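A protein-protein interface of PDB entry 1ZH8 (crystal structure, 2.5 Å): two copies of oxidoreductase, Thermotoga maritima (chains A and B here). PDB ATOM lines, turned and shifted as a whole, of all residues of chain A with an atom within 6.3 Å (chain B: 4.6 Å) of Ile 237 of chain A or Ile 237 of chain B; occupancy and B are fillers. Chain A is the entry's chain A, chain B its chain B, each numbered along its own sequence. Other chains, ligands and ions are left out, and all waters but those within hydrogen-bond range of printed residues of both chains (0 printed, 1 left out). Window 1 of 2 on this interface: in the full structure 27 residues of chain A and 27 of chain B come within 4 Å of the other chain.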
ATOM      1  N   PHE A 165      -5.157 -24.622  -8.448  1.00  0.00           N
ATOM      2  CA  PHE A 165      -4.041 -23.677  -8.614  1.00  0.00           C
ATOM      3  C   PHE A 165      -2.853 -24.026  -7.706  1.00  0.00           C
ATOM      4  O   PHE A 165      -3.019 -24.194  -6.498  1.00  0.00           O
ATOM      5  CB  PHE A 165      -4.531 -22.245  -8.311  1.00  0.00           C
ATOM      6  CG  PHE A 165      -3.437 -21.193  -8.272  1.00  0.00           C
ATOM      7  CD1 PHE A 165      -2.839 -20.741  -9.443  1.00  0.00           C
ATOM      8  CD2 PHE A 165      -3.030 -20.630  -7.065  1.00  0.00           C
ATOM      9  CE1 PHE A 165      -1.838 -19.752  -9.406  1.00  0.00           C
ATOM     10  CE2 PHE A 165      -2.017 -19.657  -7.016  1.00  0.00           C
ATOM     11  CZ  PHE A 165      -1.427 -19.211  -8.188  1.00  0.00           C
ATOM     12  N   TRP A 216       1.072 -26.463 -21.494  1.00  0.00           N
ATOM     13  CA  TRP A 216       1.604 -25.244 -22.072  1.00  0.00           C
ATOM     14  C   TRP A 216       2.107 -24.340 -20.970  1.00  0.00           C
ATOM     15  O   TRP A 216       1.609 -24.401 -19.837  1.00  0.00           O
ATOM     16  CB  TRP A 216       0.554 -24.521 -22.941  1.00  0.00           C
ATOM     17  CG  TRP A 216      -0.645 -24.033 -22.181  1.00  0.00           C
ATOM     18  CD1 TRP A 216      -1.861 -24.650 -22.091  1.00  0.00           C
ATOM     19  CD2 TRP A 216      -0.758 -22.817 -21.408  1.00  0.00           C
ATOM     20  NE1 TRP A 216      -2.723 -23.900 -21.316  1.00  0.00           N
ATOM     21  CE2 TRP A 216      -2.066 -22.777 -20.878  1.00  0.00           C
ATOM     22  CE3 TRP A 216       0.119 -21.759 -21.119  1.00  0.00           C
ATOM     23  CZ2 TRP A 216      -2.512 -21.728 -20.061  1.00  0.00           C
ATOM     24  CZ3 TRP A 216      -0.333 -20.716 -20.301  1.00  0.00           C
ATOM     25  CH2 TRP A 216      -1.631 -20.711 -19.792  1.00  0.00           C
ATOM     26  N   ILE A 217       3.072 -23.500 -21.325  1.00  0.00           N
ATOM     27  CA  ILE A 217       3.610 -22.496 -20.431  1.00  0.00           C
ATOM     28  C   ILE A 217       3.668 -21.176 -21.153  1.00  0.00           C
ATOM     29  O   ILE A 217       3.671 -21.133 -22.385  1.00  0.00           O
ATOM     30  CB  ILE A 217       5.030 -22.843 -19.980  1.00  0.00           C
ATOM     31  CG1 ILE A 217       5.956 -22.948 -21.191  1.00  0.00           C
ATOM     32  CG2 ILE A 217       5.046 -24.162 -19.280  1.00  0.00           C
ATOM     33  CD1 ILE A 217       6.542 -21.638 -21.669  1.00  0.00           C
ATOM     34  N   SER A 218       3.756 -20.104 -20.371  1.00  0.00           N
ATOM     35  CA  SER A 218       3.977 -18.760 -20.875  1.00  0.00           C
ATOM     36  C   SER A 218       4.849 -18.136 -19.797  1.00  0.00           C
ATOM     37  O   SER A 218       4.485 -18.154 -18.632  1.00  0.00           O
ATOM     38  CB  SER A 218       2.628 -18.043 -21.005  1.00  0.00           C
ATOM     39  OG  SER A 218       2.769 -16.652 -21.257  1.00  0.00           O
ATOM     40  N   ALA A 219       6.017 -17.617 -20.141  1.00  0.00           N
ATOM     41  CA  ALA A 219       6.954 -17.215 -19.101  1.00  0.00           C
ATOM     42  C   ALA A 219       7.821 -16.057 -19.509  1.00  0.00           C
ATOM     43  O   ALA A 219       8.045 -15.823 -20.697  1.00  0.00           O
ATOM     44  CB  ALA A 219       7.836 -18.410 -18.697  1.00  0.00           C
ATOM     45  N   VAL A 220       8.340 -15.342 -18.520  1.00  0.00           N
ATOM     46  CA  VAL A 220       9.293 -14.268 -18.793  1.00  0.00           C
ATOM     47  C   VAL A 220      10.582 -14.493 -17.976  1.00  0.00           C
ATOM     48  O   VAL A 220      10.540 -14.626 -16.752  1.00  0.00           O
ATOM     49  CB  VAL A 220       8.639 -12.868 -18.573  1.00  0.00           C
ATOM     50  CG1 VAL A 220       8.020 -12.786 -17.211  1.00  0.00           C
ATOM     51  CG2 VAL A 220       9.637 -11.741 -18.756  1.00  0.00           C
ATOM     52  N   SER A 235       9.554 -15.968 -14.282  1.00  0.00           N
ATOM     53  CA  SER A 235       8.159 -16.039 -13.821  1.00  0.00           C
ATOM     54  C   SER A 235       7.286 -16.657 -14.910  1.00  0.00           C
ATOM     55  O   SER A 235       7.385 -16.282 -16.094  1.00  0.00           O
ATOM     56  CB  SER A 235       7.636 -14.665 -13.433  1.00  0.00           C
ATOM     57  OG  SER A 235       6.472 -14.782 -12.639  1.00  0.00           O
ATOM     58  N   SER A 236       6.423 -17.587 -14.515  1.00  0.00           N
ATOM     59  CA  SER A 236       5.673 -18.390 -15.476  1.00  0.00           C
ATOM     60  C   SER A 236       4.262 -18.733 -15.030  1.00  0.00           C
ATOM     61  O   SER A 236       3.997 -18.883 -13.840  1.00  0.00           O
ATOM     62  CB  SER A 236       6.418 -19.695 -15.738  1.00  0.00           C
ATOM     63  OG  SER A 236       6.429 -20.481 -14.573  1.00  0.00           O
ATOM     64  N   ILE A 237       3.358 -18.853 -15.998  1.00  0.00           N
ATOM     65  CA  ILE A 237       2.093 -19.561 -15.781  1.00  0.00           C
ATOM     66  C   ILE A 237       2.042 -20.732 -16.721  1.00  0.00           C
ATOM     67  O   ILE A 237       2.636 -20.720 -17.813  1.00  0.00           O
ATOM     68  CB  ILE A 237       0.837 -18.718 -16.059  1.00  0.00           C
ATOM     69  CG1 ILE A 237       1.040 -17.852 -17.286  1.00  0.00           C
ATOM     70  CG2 ILE A 237       0.479 -17.855 -14.861  1.00  0.00           C
ATOM     71  CD1 ILE A 237      -0.243 -17.292 -17.796  1.00  0.00           C
ATOM     72  N   PHE A 238       1.298 -21.736 -16.319  1.00  0.00           N
ATOM     73  CA  PHE A 238       1.165 -22.911 -17.144  1.00  0.00           C
ATOM     74  C   PHE A 238      -0.103 -23.648 -16.723  1.00  0.00           C
ATOM     75  O   PHE A 238      -0.737 -23.318 -15.723  1.00  0.00           O
ATOM     76  CB  PHE A 238       2.411 -23.815 -17.017  1.00  0.00           C
ATOM     77  CG  PHE A 238       2.855 -24.046 -15.594  1.00  0.00           C
ATOM     78  CD1 PHE A 238       3.614 -23.069 -14.910  1.00  0.00           C
ATOM     79  CD2 PHE A 238       2.520 -25.217 -14.930  1.00  0.00           C
ATOM     80  CE1 PHE A 238       4.045 -23.255 -13.606  1.00  0.00           C
ATOM     81  CE2 PHE A 238       2.954 -25.426 -13.603  1.00  0.00           C
ATOM     82  CZ  PHE A 238       3.723 -24.446 -12.942  1.00  0.00           C
ATOM     83  N   GLU A 239      -0.474 -24.643 -17.505  1.00  0.00           N
ATOM     84  CA  GLU A 239      -1.623 -25.447 -17.177  1.00  0.00           C
ATOM     85  C   GLU A 239      -1.174 -26.898 -17.292  1.00  0.00           C
ATOM     86  O   GLU A 239      -0.481 -27.273 -18.228  1.00  0.00           O
ATOM     87  CB  GLU A 239      -2.771 -25.104 -18.126  1.00  0.00           C
ATOM     88  CG  GLU A 239      -4.074 -25.805 -17.850  1.00  0.00           C
ATOM     89  CD  GLU A 239      -5.217 -25.312 -18.750  1.00  0.00           C
ATOM     90  OE1 GLU A 239      -4.960 -24.609 -19.752  1.00  0.00           O
ATOM     91  OE2 GLU A 239      -6.384 -25.638 -18.448  1.00  0.00           O
ATOM     92  N   VAL A 245      -3.966 -25.042 -12.871  1.00  0.00           N
ATOM     93  CA  VAL A 245      -3.146 -23.886 -13.245  1.00  0.00           C
ATOM     94  C   VAL A 245      -1.953 -23.755 -12.301  1.00  0.00           C
ATOM     95  O   VAL A 245      -2.083 -23.906 -11.069  1.00  0.00           O
ATOM     96  CB  VAL A 245      -3.971 -22.584 -13.215  1.00  0.00           C
ATOM     97  CG1 VAL A 245      -3.091 -21.356 -13.559  1.00  0.00           C
ATOM     98  CG2 VAL A 245      -5.200 -22.691 -14.136  1.00  0.00           C
ATOM     99  N   GLY A 246      -0.788 -23.489 -12.876  1.00  0.00           N
ATOM    100  CA  GLY A 246       0.418 -23.307 -12.095  1.00  0.00           C
ATOM    101  C   GLY A 246       1.026 -21.935 -12.262  1.00  0.00           C
ATOM    102  O   GLY A 246       0.911 -21.321 -13.330  1.00  0.00           O
ATOM    103  N   ASN A 247       1.658 -21.448 -11.193  1.00  0.00           N
ATOM    104  CA  ASN A 247       2.565 -20.295 -11.239  1.00  0.00           C
ATOM    105  C   ASN A 247       3.898 -20.720 -10.653  1.00  0.00           C
ATOM    106  O   ASN A 247       3.967 -21.230  -9.539  1.00  0.00           O
ATOM    107  CB  ASN A 247       2.050 -19.102 -10.412  1.00  0.00           C
ATOM    108  CG  ASN A 247       0.870 -18.378 -11.051  1.00  0.00           C
ATOM    109  OD1 ASN A 247       0.281 -18.839 -12.041  1.00  0.00           O
ATOM    110  ND2 ASN A 247       0.513 -17.224 -10.478  1.00  0.00           N
ATOM    111  N   TYR A 248       4.970 -20.491 -11.376  1.00  0.00           N
ATOM    112  CA  TYR A 248       6.275 -20.834 -10.860  1.00  0.00           C
ATOM    113  C   TYR A 248       7.151 -19.627 -11.119  1.00  0.00           C
ATOM    114  O   TYR A 248       7.316 -19.236 -12.290  1.00  0.00           O
ATOM    115  CB  TYR A 248       6.810 -22.089 -11.559  1.00  0.00           C
ATOM    116  CG  TYR A 248       8.309 -22.313 -11.457  1.00  0.00           C
ATOM    117  CD1 TYR A 248       8.917 -22.629 -10.238  1.00  0.00           C
ATOM    118  CD2 TYR A 248       9.112 -22.249 -12.594  1.00  0.00           C
ATOM    119  CE1 TYR A 248      10.274 -22.840 -10.161  1.00  0.00           C
ATOM    120  CE2 TYR A 248      10.486 -22.481 -12.532  1.00  0.00           C
ATOM    121  CZ  TYR A 248      11.061 -22.770 -11.313  1.00  0.00           C
ATOM    122  OH  TYR A 248      12.418 -23.002 -11.249  1.00  0.00           O
ATOM    123  N   THR A 249       7.658 -19.029 -10.029  1.00  0.00           N
ATOM    124  CA  THR A 249       8.524 -17.838 -10.078  1.00  0.00           C
ATOM    125  C   THR A 249       9.783 -18.080  -9.238  1.00  0.00           C
ATOM    126  O   THR A 249       9.699 -18.568  -8.105  1.00  0.00           O
ATOM    127  CB  THR A 249       7.801 -16.598  -9.529  1.00  0.00           C
ATOM    128  OG1 THR A 249       6.698 -16.295 -10.367  1.00  0.00           O
ATOM    129  CG2 THR A 249       8.697 -15.403  -9.494  1.00  0.00           C
ATOM    130  N   SER A 329       9.874 -18.720 -24.178  1.00  0.00           N
ATOM    131  CA  SER A 329       8.521 -18.151 -24.253  1.00  0.00           C
ATOM    132  C   SER A 329       8.469 -16.649 -24.518  1.00  0.00           C
ATOM    133  O   SER A 329       7.677 -16.205 -25.333  1.00  0.00           O
ATOM    134  CB  SER A 329       7.700 -18.460 -23.000  1.00  0.00           C
ATOM    135  OG  SER A 329       6.503 -17.667 -22.995  1.00  0.00           O
ATOM    136  N   GLY A 331       6.963 -14.720 -22.917  1.00  0.00           N
ATOM    137  CA  GLY A 331       5.571 -14.430 -22.642  1.00  0.00           C
ATOM    138  C   GLY A 331       4.603 -15.047 -23.623  1.00  0.00           C
ATOM    139  O   GLY A 331       3.393 -14.964 -23.439  1.00  0.00           O
ATOM    140  N   TRP B 216       2.069  -5.959 -21.521  1.00  0.00           N
ATOM    141  CA  TRP B 216       1.516  -7.225 -22.003  1.00  0.00           C
ATOM    142  C   TRP B 216       1.157  -8.134 -20.859  1.00  0.00           C
ATOM    143  O   TRP B 216       1.800  -8.133 -19.800  1.00  0.00           O
ATOM    144  CB  TRP B 216       2.445  -7.943 -23.009  1.00  0.00           C
ATOM    145  CG  TRP B 216       3.714  -8.425 -22.412  1.00  0.00           C
ATOM    146  CD1 TRP B 216       4.917  -7.791 -22.447  1.00  0.00           C
ATOM    147  CD2 TRP B 216       3.917  -9.638 -21.666  1.00  0.00           C
ATOM    148  NE1 TRP B 216       5.863  -8.527 -21.767  1.00  0.00           N
ATOM    149  CE2 TRP B 216       5.273  -9.663 -21.272  1.00  0.00           C
ATOM    150  CE3 TRP B 216       3.084 -10.701 -21.284  1.00  0.00           C
ATOM    151  CZ2 TRP B 216       5.824 -10.719 -20.521  1.00  0.00           C
ATOM    152  CZ3 TRP B 216       3.639 -11.753 -20.521  1.00  0.00           C
ATOM    153  CH2 TRP B 216       4.986 -11.751 -20.161  1.00  0.00           C
ATOM    154  N   ILE B 217       0.112  -8.906 -21.084  1.00  0.00           N
ATOM    155  CA  ILE B 217      -0.323  -9.888 -20.123  1.00  0.00           C
ATOM    156  C   ILE B 217      -0.388 -11.207 -20.847  1.00  0.00           C
ATOM    157  O   ILE B 217      -0.455 -11.264 -22.083  1.00  0.00           O
ATOM    158  CB  ILE B 217      -1.713  -9.561 -19.586  1.00  0.00           C
ATOM    159  CG1 ILE B 217      -2.741  -9.574 -20.720  1.00  0.00           C
ATOM    160  CG2 ILE B 217      -1.750  -8.159 -19.027  1.00  0.00           C
ATOM    161  CD1 ILE B 217      -3.400 -10.916 -20.988  1.00  0.00           C
ATOM    162  N   SER B 218      -0.373 -12.273 -20.065  1.00  0.00           N
ATOM    163  CA  SER B 218      -0.669 -13.607 -20.550  1.00  0.00           C
ATOM    164  C   SER B 218      -1.419 -14.212 -19.368  1.00  0.00           C
ATOM    165  O   SER B 218      -0.978 -14.095 -18.221  1.00  0.00           O
ATOM    166  CB  SER B 218       0.638 -14.332 -20.895  1.00  0.00           C
ATOM    167  OG  SER B 218       0.442 -15.730 -21.059  1.00  0.00           O
ATOM    168  N   ALA B 219      -2.576 -14.810 -19.623  1.00  0.00           N
ATOM    169  CA  ALA B 219      -3.497 -15.140 -18.541  1.00  0.00           C
ATOM    170  C   ALA B 219      -4.407 -16.313 -18.890  1.00  0.00           C
ATOM    171  O   ALA B 219      -4.705 -16.564 -20.059  1.00  0.00           O
ATOM    172  CB  ALA B 219      -4.349 -13.913 -18.191  1.00  0.00           C
ATOM    173  N   SER B 235      -5.712 -16.321 -13.439  1.00  0.00           N
ATOM    174  CA  SER B 235      -4.291 -16.272 -13.129  1.00  0.00           C
ATOM    175  C   SER B 235      -3.546 -15.683 -14.338  1.00  0.00           C
ATOM    176  O   SER B 235      -3.799 -16.077 -15.496  1.00  0.00           O
ATOM    177  CB  SER B 235      -3.767 -17.665 -12.813  1.00  0.00           C
ATOM    178  OG  SER B 235      -2.489 -17.585 -12.208  1.00  0.00           O
ATOM    179  N   SER B 236      -2.633 -14.756 -14.069  1.00  0.00           N
ATOM    180  CA  SER B 236      -1.970 -14.013 -15.117  1.00  0.00           C
ATOM    181  C   SER B 236      -0.516 -13.668 -14.801  1.00  0.00           C
ATOM    182  O   SER B 236      -0.131 -13.515 -13.642  1.00  0.00           O
ATOM    183  CB  SER B 236      -2.721 -12.710 -15.388  1.00  0.00           C
ATOM    184  OG  SER B 236      -2.693 -11.877 -14.239  1.00  0.00           O
ATOM    185  N   ILE B 237       0.275 -13.518 -15.854  1.00  0.00           N
ATOM    186  CA  ILE B 237       1.605 -12.923 -15.753  1.00  0.00           C
ATOM    187  C   ILE B 237       1.632 -11.726 -16.694  1.00  0.00           C
ATOM    188  O   ILE B 237       0.958 -11.720 -17.718  1.00  0.00           O
ATOM    189  CB  ILE B 237       2.761 -13.892 -16.051  1.00  0.00           C
ATOM    190  CG1 ILE B 237       2.669 -14.461 -17.464  1.00  0.00           C
ATOM    191  CG2 ILE B 237       2.820 -14.997 -14.998  1.00  0.00           C
ATOM    192  CD1 ILE B 237       3.962 -15.069 -17.906  1.00  0.00           C
ATOM    193  N   PHE B 238       2.363 -10.694 -16.322  1.00  0.00           N
ATOM    194  CA  PHE B 238       2.419  -9.529 -17.159  1.00  0.00           C
ATOM    195  C   PHE B 238       3.694  -8.750 -16.861  1.00  0.00           C
ATOM    196  O   PHE B 238       4.375  -9.011 -15.870  1.00  0.00           O
ATOM    197  CB  PHE B 238       1.150  -8.666 -16.956  1.00  0.00           C
ATOM    198  CG  PHE B 238       0.836  -8.381 -15.513  1.00  0.00           C
ATOM    199  CD1 PHE B 238       0.111  -9.287 -14.749  1.00  0.00           C
ATOM    200  CD2 PHE B 238       1.270  -7.200 -14.912  1.00  0.00           C
ATOM    201  CE1 PHE B 238      -0.180  -9.018 -13.397  1.00  0.00           C
ATOM    202  CE2 PHE B 238       0.974  -6.925 -13.558  1.00  0.00           C
ATOM    203  CZ  PHE B 238       0.260  -7.829 -12.804  1.00  0.00           C
ATOM    204  N   GLY B 246       4.764  -8.962 -13.136  1.00  0.00           N
ATOM    205  CA  GLY B 246       3.650  -9.109 -12.224  1.00  0.00           C
ATOM    206  C   GLY B 246       2.975 -10.445 -12.387  1.00  0.00           C
ATOM    207  O   GLY B 246       2.972 -11.023 -13.486  1.00  0.00           O
ATOM    208  N   ASN B 247       2.435 -10.943 -11.274  1.00  0.00           N
ATOM    209  CA  ASN B 247       1.515 -12.052 -11.266  1.00  0.00           C
ATOM    210  C   ASN B 247       0.265 -11.609 -10.527  1.00  0.00           C
ATOM    211  O   ASN B 247       0.328 -11.013  -9.449  1.00  0.00           O
ATOM    212  CB  ASN B 247       2.070 -13.276 -10.522  1.00  0.00           C
ATOM    213  CG  ASN B 247       3.297 -13.898 -11.187  1.00  0.00           C
ATOM    214  OD1 ASN B 247       3.741 -13.477 -12.260  1.00  0.00           O
ATOM    215  ND2 ASN B 247       3.859 -14.909 -10.528  1.00  0.00           N
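The side-chain hydroxyl of Ser 218 of chain A sits at hydrogen-bond distance from the side-chain hydroxyl of Ser 218 of chain B, 2.5 Å away.
The side-chain hydroxyl of Ser 235 of chain A lies within hydrogen-bond range of the side-chain amide oxygen of Asn 247 of chain B (3.1 Å).
The side-chain hydroxyl of Ser 235 of chain B sits at hydrogen-bond distance from the side-chain amide oxygen of Asn 247 of chain A, at 3.0 Å.
OG1 of Thr 249 of chain A lies within hydrogen-bond range of ND2 of Asn 247 of chain B (3.2 Å).
N of Ser 218 of chain A is in hydrogen-bond range of O of Ile 237 of chain A, 2.9 Å away.
The side-chain hydroxyl (OG) of Ser 218 of chain A sits at hydrogen-bond distance from the backbone carbonyl oxygen (O) of Gly 331 of chain A, 2.8 Å away.
The backbone NH (N) of Val 220 of chain A is in hydrogen-bond range of the backbone carbonyl oxygen (O) of Ser 235 of chain A (2.8 Å).
The side-chain hydroxyl of Ser 235 of chain A lies within hydrogen-bond range of the side-chain hydroxyl of Thr 249 of chain A (2.7 Å).
The side-chain hydroxyl (OG) of Ser 329 of chain A sits close to the backbone NH (N) of Gly 331 of chain A (3.0 Å).
The backbone NH of Ile 237 of chain B lies within hydrogen-bond range of the backbone carbonyl oxygen of Ser 218 of chain B (2.7 Å).
Among the printed residues, merely in contact across the chains: Phe 165 of chain A with Ser 235 of chain B, Ser 218 of chain A with Ile 237 of chain B, Ala 219 of chain A with Ile 237 of chain B, Ile 237 of chain A with Ser 218 of chain B, Ile 237 of chain A with Ala 219 of chain B, Ile 237 of chain A with Ser 235 of chain B, Ile 237 of chain A with Ile 237 of chain B, Val 245 of chain A with Ser 235 of chain B, Gly 331 of chain A with Trp 216 of chain B and Gly 331 of chain A with Ser 218 of chain B.
Printed residues of chain B within 4 Å of Ile 237 of chain A: Ser 218 (3.3 Å), Ala 219 (3.9 Å), Ser 235 (3.99 Å) and Ile 237 (3.7 Å).
Printed residues of chain A within 4 Å of Ile 237 of chain B: Ser 218, Ala 219 and Ile 237.
Of the printed residues of chain A, Ala 219 of chain B touches Ile 237 (3.9 Å).
Of the printed residues of chain A, Asn 247 of chain B touches Ser 235 (3.1 Å) and Thr 249 (3.2 Å).
Of the printed residues of chain B, Ser 218 of chain A touches Ser 218 (2.5 Å) and Ile 237 (3.2 Å).
Printed residues of chain A within 4 Å of Trp 216 of chain B: Gly 331.
The nearest printed residue of chain A that does not touch Ile 237 of chain B is Ser 236 of chain A (4.005 Å).
The nearest printed residue of chain B that does not touch Val 245 of chain A is Ser 236 of chain B (6.6 Å).
Of the 18 printed residues of chain A, 9 touch a printed residue of chain B.
Hydrophobic or aromatic side chains of chain A that line the printed part of chain B: Phe 165, Ile 237 and Val 245.
Along chain A the printed residues that touch a printed residue of chain B span positions 165 to 331.
Of the 10 printed residues of chain B, 6 touch a printed residue of chain A.
Hydrophobic or aromatic side chains of chain B that line the printed part of chain A: Trp 216 and Ile 237.
Along chain B the printed residues that touch a printed residue of chain A span positions 216 to 247.
Among the printed residues, 14 pairs touch across the chains.
Among the printed residues, no Asp or Glu carboxylate lies within 4 Å of a Lys or Arg side-chain nitrogen of the other chain.
Ser 218 of chain A touches Ile 237 of chain B, and with the chains exchanged Ile 237 of chain A touches Ser 218 of chain B.
Ser 235 of chain A touches Asn 247 of chain B, and with the chains exchanged Asn 247 of chain A touches Ser 235 of chain B.
Ile 237 of chain A touches Ser 235 of chain B, but with the chains exchanged Ser 235 of chain A does not touch Ile 237 of chain B (4.1 Å).
Ile 237 of chain B touches its own counterpart, Ile 237 of chain A.
10 positions are printed for both chains.
Of the 14 pairs that touch across the chains among the printed residues, 8 have their exchanged pair printed and touching as well.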
